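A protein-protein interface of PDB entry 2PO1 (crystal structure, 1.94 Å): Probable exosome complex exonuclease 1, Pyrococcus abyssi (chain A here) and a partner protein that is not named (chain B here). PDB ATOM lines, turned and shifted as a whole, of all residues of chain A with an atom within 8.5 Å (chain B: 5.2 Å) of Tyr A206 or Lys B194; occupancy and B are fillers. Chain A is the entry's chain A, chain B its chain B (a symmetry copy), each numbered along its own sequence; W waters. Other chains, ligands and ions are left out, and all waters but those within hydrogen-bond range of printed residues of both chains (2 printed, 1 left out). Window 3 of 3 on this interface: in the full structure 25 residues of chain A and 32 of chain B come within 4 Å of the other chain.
O of Leu A207 lies within hydrogen-bond range of N of Ile B234 (2.6 Å).
The side-chain hydroxyl of Thr B231 lies within hydrogen-bond range of the side-chain hydroxyl of Tyr A206, 2.8 Å away.
The side-chain hydroxyl of Tyr A206 is in hydrogen-bond range of the side-chain carboxylate of Asp B229.
The backbone carbonyl oxygen (O) of Gly A205 sits close to the backbone carbonyl oxygen (O) of Ser B235, at 3.1 Å.
O of Ser B120 sits at hydrogen-bond distance from NZ of Lys B194, at 3.0 Å.
The backbone NH of Tyr A206 sits at hydrogen-bond distance from the backbone carbonyl oxygen of Glu A184 (3.2 Å).
OG of Ser B120 sits close to N of Ala B122, at 3.2 Å.
The backbone NH (N) of Asp A186 is in hydrogen-bond range of the backbone carbonyl oxygen (O) of Asp A204 (2.7 Å).
The side-chain carboxylate (OD2) of Asp B229 sits at hydrogen-bond distance from the side-chain hydroxyl (OG1) of Thr B231 (2.5 Å).
OD2 of Asp B229 is in hydrogen-bond range of N of His B233, at 3.2 Å.
Met A203 touches Ile B234 (CE to O, 2.9 Å).
OD1 of Asp A204 touches CG of Glu B119 (3.3 Å).
Glu B119 touches Tyr A206.
Ser B120 touches Tyr A206 (CA to CD1, 3.5 Å).
Tyr A206 touches His B233 (CZ to CB, 3.2 Å).
Tyr A206 touches Ile B234.
Tyr A206 touches Ser B235 (CD1 to CB, 3.99 Å).
Leu A207 touches His B233.
O of Thr A208 touches CD1 of Ile B234, 3.8 Å away.
CD1 of Ile B234 touches CA of Lys A209, at 3.7 Å.
Of the printed residues of chain B, Tyr A206 touches Glu B119, Ser B120, Lys B194, Asp B229, Thr B231, His B233, Ile B234 and Ser B235.
Of the printed residues of chain A, Lys B194 touches Tyr A206 (3.5 Å).
Of the printed residues of chain A, Ser B235 touches Met A203, Gly A205 and Tyr A206.
Printed residues of chain A within 4 Å of Glu B119: Asp A204 (3.3 Å), Gly A205 (3.2 Å) and Tyr A206 (3.5 Å).
Printed residues of chain A within 4 Å of Ile B234: Met A203 (2.9 Å), Gly A205 (3.6 Å), Tyr A206 (3.2 Å), Leu A207 (2.6 Å), Thr A208 (3.8 Å), Lys A209 (3.7 Å) and Phe A212 (3.4 Å).
Of the printed residues of chain B, Thr A208 touches His B233 and Ile B234.
Of the printed residues of chain A, Ser B120 touches Tyr A206 (3.5 Å).
Asp A186 touches none of the printed residues of chain B.
The nearest printed residue of chain B that does not touch Tyr A206 is Lys B121 (5.7 Å).
The nearest printed residue of chain A that does not touch Lys B194 is Gly A205 (9.5 Å).
Of the 16 printed residues of chain A, 8 touch a printed residue of chain B.
Printed residues of chain B that touch a printed residue of chain A: Glu B119, Ser B120, Lys B194, Asp B229, Thr B231, His B233, Ile B234 and Ser B235.
Among the printed residues, no Asp or Glu carboxylate lies within 4 Å of a Lys or Arg side-chain nitrogen of the other chain.
Water W2 lies within hydrogen-bond range of the side-chain carboxylate of Glu B119 (2.7 Å) and the side-chain carboxylate of Asp A204 (3.3 Å).
Water W1 lies within hydrogen-bond range of the side-chain hydroxyl of Tyr A206 (2.8 Å) and the side-chain hydroxyl of Thr B231 (3.0 Å).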
ATOM      1  N   LYS A 166     -15.666 -39.154 -25.540  1.00  0.00           N
ATOM      2  CA  LYS A 166     -16.695 -39.257 -26.561  1.00  0.00           C
ATOM      3  C   LYS A 166     -16.018 -39.092 -27.911  1.00  0.00           C
ATOM      4  O   LYS A 166     -15.294 -38.124 -28.131  1.00  0.00           O
ATOM      5  CB  LYS A 166     -17.835 -38.248 -26.338  1.00  0.00           C
ATOM      6  CG  LYS A 166     -18.853 -38.278 -27.395  1.00  0.00           C
ATOM      7  CD  LYS A 166     -20.076 -37.534 -26.992  1.00  0.00           C
ATOM      8  CE  LYS A 166     -20.883 -37.230 -28.202  1.00  0.00           C
ATOM      9  NZ  LYS A 166     -21.640 -35.975 -28.055  1.00  0.00           N
ATOM     10  N   ILE A 171     -19.662 -42.866 -26.473  1.00  0.00           N
ATOM     11  CA  ILE A 171     -18.878 -42.911 -25.254  1.00  0.00           C
ATOM     12  C   ILE A 171     -17.878 -44.063 -25.362  1.00  0.00           C
ATOM     13  O   ILE A 171     -18.278 -45.202 -25.502  1.00  0.00           O
ATOM     14  CB  ILE A 171     -19.794 -43.158 -24.070  1.00  0.00           C
ATOM     15  CG1 ILE A 171     -20.925 -42.120 -24.029  1.00  0.00           C
ATOM     16  CG2 ILE A 171     -18.962 -43.296 -22.780  1.00  0.00           C
ATOM     17  CD1 ILE A 171     -20.493 -40.693 -24.028  1.00  0.00           C
ATOM     18  N   GLY A 183     -11.867 -35.809 -30.862  1.00  0.00           N
ATOM     19  CA  GLY A 183     -12.938 -36.323 -30.034  1.00  0.00           C
ATOM     20  C   GLY A 183     -13.850 -35.230 -29.535  1.00  0.00           C
ATOM     21  O   GLY A 183     -13.521 -34.044 -29.615  1.00  0.00           O
ATOM     22  N   GLU A 184     -14.967 -35.616 -28.948  1.00  0.00           N
ATOM     23  CA  GLU A 184     -15.841 -34.599 -28.379  1.00  0.00           C
ATOM     24  C   GLU A 184     -15.700 -34.332 -26.878  1.00  0.00           C
ATOM     25  O   GLU A 184     -16.185 -33.323 -26.374  1.00  0.00           O
ATOM     26  CB  GLU A 184     -17.264 -34.941 -28.690  1.00  0.00           C
ATOM     27  CG  GLU A 184     -17.442 -34.995 -30.180  1.00  0.00           C
ATOM     28  CD  GLU A 184     -18.393 -36.066 -30.559  1.00  0.00           C
ATOM     29  OE1 GLU A 184     -19.537 -35.694 -30.843  1.00  0.00           O
ATOM     30  OE2 GLU A 184     -18.038 -37.272 -30.539  1.00  0.00           O
ATOM     31  N   ALA A 185     -15.048 -35.231 -26.168  1.00  0.00           N
ATOM     32  CA  ALA A 185     -14.934 -35.088 -24.698  1.00  0.00           C
ATOM     33  C   ALA A 185     -13.864 -36.039 -24.277  1.00  0.00           C
ATOM     34  O   ALA A 185     -13.749 -37.113 -24.857  1.00  0.00           O
ATOM     35  CB  ALA A 185     -16.229 -35.501 -24.025  1.00  0.00           C
ATOM     36  N   ASP A 186     -13.186 -35.697 -23.189  1.00  0.00           N
ATOM     37  CA  ASP A 186     -12.234 -36.556 -22.557  1.00  0.00           C
ATOM     38  C   ASP A 186     -12.604 -36.424 -21.076  1.00  0.00           C
ATOM     39  O   ASP A 186     -12.868 -35.299 -20.572  1.00  0.00           O
ATOM     40  CB  ASP A 186     -10.819 -36.012 -22.850  1.00  0.00           C
ATOM     41  CG  ASP A 186      -9.689 -36.893 -22.270  1.00  0.00           C
ATOM     42  OD1 ASP A 186      -8.580 -36.338 -22.046  1.00  0.00           O
ATOM     43  OD2 ASP A 186      -9.867 -38.118 -22.056  1.00  0.00           O
ATOM     44  N   VAL A 187     -12.689 -37.570 -20.416  1.00  0.00           N
ATOM     45  CA  VAL A 187     -13.132 -37.673 -19.008  1.00  0.00           C
ATOM     46  C   VAL A 187     -12.204 -38.628 -18.268  1.00  0.00           C
ATOM     47  O   VAL A 187     -12.490 -39.877 -18.178  1.00  0.00           O
ATOM     48  CB  VAL A 187     -14.600 -38.207 -18.872  1.00  0.00           C
ATOM     49  CG1 VAL A 187     -15.059 -38.150 -17.437  1.00  0.00           C
ATOM     50  CG2 VAL A 187     -15.532 -37.390 -19.700  1.00  0.00           C
ATOM     51  N   MET A 203     -13.495 -33.226 -16.983  1.00  0.00           N
ATOM     52  CA  MET A 203     -14.179 -33.375 -18.238  1.00  0.00           C
ATOM     53  C   MET A 203     -13.816 -32.183 -19.105  1.00  0.00           C
ATOM     54  O   MET A 203     -14.011 -31.034 -18.731  1.00  0.00           O
ATOM     55  CB  MET A 203     -15.679 -33.476 -18.014  1.00  0.00           C
ATOM     56  CG  MET A 203     -16.459 -33.896 -19.238  1.00  0.00           C
ATOM     57  SD  MET A 203     -16.694 -32.548 -20.374  1.00  0.00           S
ATOM     58  CE  MET A 203     -18.178 -31.825 -19.788  1.00  0.00           C
ATOM     59  N   ASP A 204     -13.234 -32.496 -20.252  1.00  0.00           N
ATOM     60  CA  ASP A 204     -12.797 -31.524 -21.235  1.00  0.00           C
ATOM     61  C   ASP A 204     -13.631 -31.894 -22.419  1.00  0.00           C
ATOM     62  O   ASP A 204     -13.464 -32.986 -22.929  1.00  0.00           O
ATOM     63  CB  ASP A 204     -11.325 -31.818 -21.577  1.00  0.00           C
ATOM     64  CG  ASP A 204     -10.708 -30.735 -22.356  1.00  0.00           C
ATOM     65  OD1 ASP A 204     -11.418 -29.732 -22.571  1.00  0.00           O
ATOM     66  OD2 ASP A 204      -9.491 -30.838 -22.721  1.00  0.00           O
ATOM     67  N   GLY A 205     -14.552 -31.033 -22.841  1.00  0.00           N
ATOM     68  CA  GLY A 205     -15.429 -31.376 -23.934  1.00  0.00           C
ATOM     69  C   GLY A 205     -16.806 -30.806 -23.731  1.00  0.00           C
ATOM     70  O   GLY A 205     -16.978 -29.765 -23.092  1.00  0.00           O
ATOM     71  N   TYR A 206     -17.804 -31.522 -24.229  1.00  0.00           N
ATOM     72  CA  TYR A 206     -19.131 -31.029 -24.176  1.00  0.00           C
ATOM     73  C   TYR A 206     -19.990 -32.260 -24.163  1.00  0.00           C
ATOM     74  O   TYR A 206     -19.995 -32.992 -25.146  1.00  0.00           O
ATOM     75  CB  TYR A 206     -19.342 -30.202 -25.428  1.00  0.00           C
ATOM     76  CG  TYR A 206     -20.550 -29.326 -25.451  1.00  0.00           C
ATOM     77  CD1 TYR A 206     -20.616 -28.187 -24.648  1.00  0.00           C
ATOM     78  CD2 TYR A 206     -21.603 -29.597 -26.319  1.00  0.00           C
ATOM     79  CE1 TYR A 206     -21.705 -27.364 -24.694  1.00  0.00           C
ATOM     80  CE2 TYR A 206     -22.689 -28.771 -26.381  1.00  0.00           C
ATOM     81  CZ  TYR A 206     -22.729 -27.648 -25.565  1.00  0.00           C
ATOM     82  OH  TYR A 206     -23.790 -26.830 -25.582  1.00  0.00           O
ATOM     83  N   LEU A 207     -20.663 -32.533 -23.038  1.00  0.00           N
ATOM     84  CA  LEU A 207     -21.501 -33.734 -22.918  1.00  0.00           C
ATOM     85  C   LEU A 207     -22.844 -33.389 -22.330  1.00  0.00           C
ATOM     86  O   LEU A 207     -23.002 -32.329 -21.749  1.00  0.00           O
ATOM     87  CB  LEU A 207     -20.816 -34.738 -22.009  1.00  0.00           C
ATOM     88  CG  LEU A 207     -19.434 -35.202 -22.452  1.00  0.00           C
ATOM     89  CD1 LEU A 207     -18.798 -35.993 -21.332  1.00  0.00           C
ATOM     90  CD2 LEU A 207     -19.589 -36.073 -23.693  1.00  0.00           C
ATOM     91  N   THR A 208     -23.825 -34.283 -22.516  1.00  0.00           N
ATOM     92  CA  THR A 208     -25.079 -34.211 -21.826  1.00  0.00           C
ATOM     93  C   THR A 208     -24.744 -34.801 -20.462  1.00  0.00           C
ATOM     94  O   THR A 208     -23.667 -35.403 -20.275  1.00  0.00           O
ATOM     95  CB  THR A 208     -26.163 -35.099 -22.503  1.00  0.00           C
ATOM     96  OG1 THR A 208     -25.699 -36.461 -22.558  1.00  0.00           O
ATOM     97  CG2 THR A 208     -26.440 -34.590 -23.917  1.00  0.00           C
ATOM     98  N   LYS A 209     -25.639 -34.601 -19.499  1.00  0.00           N
ATOM     99  CA  LYS A 209     -25.512 -35.181 -18.157  1.00  0.00           C
ATOM    100  C   LYS A 209     -25.341 -36.684 -18.253  1.00  0.00           C
ATOM    101  O   LYS A 209     -24.457 -37.268 -17.601  1.00  0.00           O
ATOM    102  CB  LYS A 209     -26.771 -34.876 -17.350  1.00  0.00           C
ATOM    103  CG  LYS A 209     -26.926 -35.703 -16.083  1.00  0.00           C
ATOM    104  CD  LYS A 209     -27.946 -35.066 -15.159  1.00  0.00           C
ATOM    105  CE  LYS A 209     -29.386 -35.450 -15.525  1.00  0.00           C
ATOM    106  NZ  LYS A 209     -30.099 -35.515 -14.231  1.00  0.00           N
ATOM    107  N   GLU A 211     -24.464 -38.499 -20.942  1.00  0.00           N
ATOM    108  CA  GLU A 211     -23.161 -38.792 -21.556  1.00  0.00           C
ATOM    109  C   GLU A 211     -22.063 -38.727 -20.549  1.00  0.00           C
ATOM    110  O   GLU A 211     -21.264 -39.647 -20.456  1.00  0.00           O
ATOM    111  CB  GLU A 211     -22.823 -37.849 -22.715  1.00  0.00           C
ATOM    112  CG  GLU A 211     -23.598 -38.134 -23.961  1.00  0.00           C
ATOM    113  CD  GLU A 211     -23.362 -37.121 -25.042  1.00  0.00           C
ATOM    114  OE1 GLU A 211     -23.621 -37.473 -26.208  1.00  0.00           O
ATOM    115  OE2 GLU A 211     -22.926 -35.978 -24.738  1.00  0.00           O
ATOM    116  N   PHE A 212     -22.003 -37.630 -19.801  1.00  0.00           N
ATOM    117  CA  PHE A 212     -20.950 -37.438 -18.819  1.00  0.00           C
ATOM    118  C   PHE A 212     -20.919 -38.555 -17.797  1.00  0.00           C
ATOM    119  O   PHE A 212     -19.884 -39.172 -17.565  1.00  0.00           O
ATOM    120  CB  PHE A 212     -21.127 -36.102 -18.101  1.00  0.00           C
ATOM    121  CG  PHE A 212     -20.156 -35.912 -16.971  1.00  0.00           C
ATOM    122  CD1 PHE A 212     -20.611 -35.778 -15.671  1.00  0.00           C
ATOM    123  CD2 PHE A 212     -18.774 -35.895 -17.205  1.00  0.00           C
ATOM    124  CE1 PHE A 212     -19.745 -35.609 -14.650  1.00  0.00           C
ATOM    125  CE2 PHE A 212     -17.881 -35.728 -16.153  1.00  0.00           C
ATOM    126  CZ  PHE A 212     -18.376 -35.590 -14.886  1.00  0.00           C
ATOM    127  N   GLU B 119     -15.022 -24.985 -24.645  1.00  0.00           N
ATOM    128  CA  GLU B 119     -15.475 -26.295 -25.102  1.00  0.00           C
ATOM    129  C   GLU B 119     -16.959 -26.265 -25.313  1.00  0.00           C
ATOM    130  O   GLU B 119     -17.546 -27.161 -25.945  1.00  0.00           O
ATOM    131  CB  GLU B 119     -15.065 -27.374 -24.108  1.00  0.00           C
ATOM    132  CG  GLU B 119     -13.552 -27.620 -24.042  1.00  0.00           C
ATOM    133  CD  GLU B 119     -12.967 -27.981 -25.365  1.00  0.00           C
ATOM    134  OE1 GLU B 119     -11.876 -27.439 -25.683  1.00  0.00           O
ATOM    135  OE2 GLU B 119     -13.615 -28.782 -26.088  1.00  0.00           O
ATOM    136  N   SER B 120     -17.594 -25.220 -24.815  1.00  0.00           N
ATOM    137  CA  SER B 120     -19.000 -25.074 -25.122  1.00  0.00           C
ATOM    138  C   SER B 120     -19.136 -24.201 -26.380  1.00  0.00           C
ATOM    139  O   SER B 120     -20.234 -23.932 -26.787  1.00  0.00           O
ATOM    140  CB  SER B 120     -19.733 -24.391 -24.009  1.00  0.00           C
ATOM    141  OG  SER B 120     -19.134 -23.123 -23.842  1.00  0.00           O
ATOM    142  N   LYS B 121     -18.008 -23.699 -26.904  1.00  0.00           N
ATOM    143  CA  LYS B 121     -17.997 -22.712 -27.969  1.00  0.00           C
ATOM    144  C   LYS B 121     -18.847 -21.496 -27.621  1.00  0.00           C
ATOM    145  O   LYS B 121     -19.476 -20.884 -28.490  1.00  0.00           O
ATOM    146  CB  LYS B 121     -18.446 -23.371 -29.241  1.00  0.00           C
ATOM    147  CG  LYS B 121     -17.448 -24.400 -29.726  1.00  0.00           C
ATOM    148  CD  LYS B 121     -17.727 -24.631 -31.201  1.00  0.00           C
ATOM    149  CE  LYS B 121     -16.527 -25.206 -31.923  1.00  0.00           C
ATOM    150  NZ  LYS B 121     -16.643 -26.698 -32.002  1.00  0.00           N
ATOM    151  N   ALA B 122     -18.849 -21.152 -26.341  1.00  0.00           N
ATOM    152  CA  ALA B 122     -19.617 -20.008 -25.885  1.00  0.00           C
ATOM    153  C   ALA B 122     -19.098 -18.765 -26.544  1.00  0.00           C
ATOM    154  O   ALA B 122     -19.861 -17.885 -26.840  1.00  0.00           O
ATOM    155  CB  ALA B 122     -19.564 -19.883 -24.358  1.00  0.00           C
ATOM    156  N   ILE B 161     -18.002 -14.879 -18.407  1.00  0.00           N
ATOM    157  CA  ILE B 161     -19.005 -14.938 -19.423  1.00  0.00           C
ATOM    158  C   ILE B 161     -19.821 -13.641 -19.436  1.00  0.00           C
ATOM    159  O   ILE B 161     -20.299 -13.199 -20.502  1.00  0.00           O
ATOM    160  CB  ILE B 161     -19.911 -16.211 -19.322  1.00  0.00           C
ATOM    161  CG1 ILE B 161     -20.736 -16.365 -20.613  1.00  0.00           C
ATOM    162  CG2 ILE B 161     -20.753 -16.172 -18.105  1.00  0.00           C
ATOM    163  CD1 ILE B 161     -19.785 -16.803 -21.804  1.00  0.00           C
ATOM    164  N   VAL B 192     -20.947 -14.389 -28.854  1.00  0.00           N
ATOM    165  CA  VAL B 192     -21.170 -15.169 -27.653  1.00  0.00           C
ATOM    166  C   VAL B 192     -22.486 -15.920 -27.825  1.00  0.00           C
ATOM    167  O   VAL B 192     -23.571 -15.328 -27.940  1.00  0.00           O
ATOM    168  CB  VAL B 192     -21.225 -14.330 -26.356  1.00  0.00           C
ATOM    169  CG1 VAL B 192     -21.288 -15.252 -25.153  1.00  0.00           C
ATOM    170  CG2 VAL B 192     -20.012 -13.399 -26.229  1.00  0.00           C
ATOM    171  N   GLU B 193     -22.395 -17.234 -27.831  1.00  0.00           N
ATOM    172  CA  GLU B 193     -23.543 -18.029 -28.202  1.00  0.00           C
ATOM    173  C   GLU B 193     -24.088 -18.919 -27.127  1.00  0.00           C
ATOM    174  O   GLU B 193     -25.206 -19.380 -27.219  1.00  0.00           O
ATOM    175  CB  GLU B 193     -23.156 -18.831 -29.395  1.00  0.00           C
ATOM    176  CG  GLU B 193     -22.685 -17.894 -30.438  1.00  0.00           C
ATOM    177  CD  GLU B 193     -22.416 -18.559 -31.736  1.00  0.00           C
ATOM    178  OE1 GLU B 193     -22.265 -19.789 -31.735  1.00  0.00           O
ATOM    179  OE2 GLU B 193     -22.341 -17.834 -32.745  1.00  0.00           O
ATOM    180  N   LYS B 194     -23.322 -19.127 -26.065  1.00  0.00           N
ATOM    181  CA  LYS B 194     -23.793 -19.957 -24.974  1.00  0.00           C
ATOM    182  C   LYS B 194     -23.410 -19.234 -23.714  1.00  0.00           C
ATOM    183  O   LYS B 194     -22.565 -18.328 -23.748  1.00  0.00           O
ATOM    184  CB  LYS B 194     -23.168 -21.350 -25.084  1.00  0.00           C
ATOM    185  CG  LYS B 194     -24.104 -22.315 -25.804  1.00  0.00           C
ATOM    186  CD  LYS B 194     -23.343 -23.468 -26.389  1.00  0.00           C
ATOM    187  CE  LYS B 194     -23.874 -23.807 -27.798  1.00  0.00           C
ATOM    188  NZ  LYS B 194     -22.591 -23.831 -28.650  1.00  0.00           N
ATOM    189  N   ILE B 195     -24.053 -19.584 -22.602  1.00  0.00           N
ATOM    190  CA  ILE B 195     -23.699 -18.960 -21.334  1.00  0.00           C
ATOM    191  C   ILE B 195     -23.303 -19.978 -20.260  1.00  0.00           C
ATOM    192  O   ILE B 195     -24.038 -20.174 -19.316  1.00  0.00           O
ATOM    193  CB  ILE B 195     -24.783 -17.955 -20.815  1.00  0.00           C
ATOM    194  CG1 ILE B 195     -25.052 -16.907 -21.861  1.00  0.00           C
ATOM    195  CG2 ILE B 195     -24.310 -17.227 -19.520  1.00  0.00           C
ATOM    196  CD1 ILE B 195     -26.441 -16.346 -21.759  1.00  0.00           C
ATOM    197  N   PRO B 196     -22.113 -20.585 -20.391  1.00  0.00           N
ATOM    198  CA  PRO B 196     -21.647 -21.540 -19.409  1.00  0.00           C
ATOM    199  C   PRO B 196     -21.385 -20.837 -18.088  1.00  0.00           C
ATOM    200  O   PRO B 196     -20.867 -19.708 -18.070  1.00  0.00           O
ATOM    201  CB  PRO B 196     -20.325 -22.036 -20.016  1.00  0.00           C
ATOM    202  CG  PRO B 196     -19.851 -20.897 -20.834  1.00  0.00           C
ATOM    203  CD  PRO B 196     -21.097 -20.372 -21.443  1.00  0.00           C
ATOM    204  N   ASP B 229     -24.135 -25.112 -19.750  1.00  0.00           N
ATOM    205  CA  ASP B 229     -24.789 -24.014 -20.494  1.00  0.00           C
ATOM    206  C   ASP B 229     -26.301 -24.171 -20.553  1.00  0.00           C
ATOM    207  O   ASP B 229     -26.832 -25.151 -20.016  1.00  0.00           O
ATOM    208  CB  ASP B 229     -24.205 -23.836 -21.909  1.00  0.00           C
ATOM    209  CG  ASP B 229     -24.382 -25.052 -22.774  1.00  0.00           C
ATOM    210  OD1 ASP B 229     -23.509 -25.233 -23.650  1.00  0.00           O
ATOM    211  OD2 ASP B 229     -25.372 -25.831 -22.628  1.00  0.00           O
ATOM    212  N   GLU B 230     -26.964 -23.225 -21.230  1.00  0.00           N
ATOM    213  CA  GLU B 230     -28.436 -23.159 -21.374  1.00  0.00           C
ATOM    214  C   GLU B 230     -28.973 -24.389 -22.055  1.00  0.00           C
ATOM    215  O   GLU B 230     -30.178 -24.569 -22.114  1.00  0.00           O
ATOM    216  CB  GLU B 230     -28.851 -22.100 -22.404  1.00  0.00           C
ATOM    217  CG  GLU B 230     -28.357 -20.732 -22.265  1.00  0.00           C
ATOM    218  CD  GLU B 230     -26.992 -20.556 -22.905  1.00  0.00           C
ATOM    219  OE1 GLU B 230     -26.034 -21.021 -22.313  1.00  0.00           O
ATOM    220  OE2 GLU B 230     -26.885 -19.942 -23.967  1.00  0.00           O
ATOM    221  N   THR B 231     -28.103 -25.159 -22.697  1.00  0.00           N
ATOM    222  CA  THR B 231     -28.558 -26.176 -23.641  1.00  0.00           C
ATOM    223  C   THR B 231     -28.543 -27.544 -22.969  1.00  0.00           C
ATOM    224  O   THR B 231     -28.744 -28.550 -23.631  1.00  0.00           O
ATOM    225  CB  THR B 231     -27.727 -26.191 -24.970  1.00  0.00           C
ATOM    226  OG1 THR B 231     -26.416 -26.745 -24.748  1.00  0.00           O
ATOM    227  CG2 THR B 231     -27.549 -24.756 -25.547  1.00  0.00           C
ATOM    228  N   HIS B 233     -25.870 -28.797 -21.579  1.00  0.00           N
ATOM    229  CA  HIS B 233     -24.601 -29.481 -21.783  1.00  0.00           C
ATOM    230  C   HIS B 233     -23.612 -29.118 -20.725  1.00  0.00           C
ATOM    231  O   HIS B 233     -23.636 -28.018 -20.201  1.00  0.00           O
ATOM    232  CB  HIS B 233     -24.082 -29.240 -23.203  1.00  0.00           C
ATOM    233  CG  HIS B 233     -24.819 -30.023 -24.254  1.00  0.00           C
ATOM    234  ND1 HIS B 233     -25.960 -29.557 -24.873  1.00  0.00           N
ATOM    235  CD2 HIS B 233     -24.573 -31.239 -24.797  1.00  0.00           C
ATOM    236  CE1 HIS B 233     -26.406 -30.466 -25.725  1.00  0.00           C
ATOM    237  NE2 HIS B 233     -25.579 -31.494 -25.704  1.00  0.00           N
ATOM    238  N   ILE B 234     -22.710 -30.061 -20.421  1.00  0.00           N
ATOM    239  CA  ILE B 234     -21.640 -29.817 -19.501  1.00  0.00           C
ATOM    240  C   ILE B 234     -20.441 -29.495 -20.354  1.00  0.00           C
ATOM    241  O   ILE B 234     -20.104 -30.232 -21.277  1.00  0.00           O
ATOM    242  CB  ILE B 234     -21.353 -31.017 -18.555  1.00  0.00           C
ATOM    243  CG1 ILE B 234     -22.637 -31.543 -17.888  1.00  0.00           C
ATOM    244  CG2 ILE B 234     -20.382 -30.625 -17.497  1.00  0.00           C
ATOM    245  CD1 ILE B 234     -22.559 -33.010 -17.586  1.00  0.00           C
ATOM    246  N   SER B 235     -19.797 -28.376 -20.081  1.00  0.00           N
ATOM    247  CA  SER B 235     -18.613 -28.015 -20.874  1.00  0.00           C
ATOM    248  C   SER B 235     -17.348 -28.098 -20.063  1.00  0.00           C
ATOM    249  O   SER B 235     -16.262 -28.037 -20.620  1.00  0.00           O
ATOM    250  CB  SER B 235     -18.766 -26.612 -21.480  1.00  0.00           C
ATOM    251  OG  SER B 235     -19.041 -25.669 -20.463  1.00  0.00           O
HETATM  252  O   HOH W   1     -25.676 -26.760 -27.678  1.00  0.00           O
HETATM  253  O   HOH W   2      -9.998 -27.008 -23.824  1.00  0.00           O
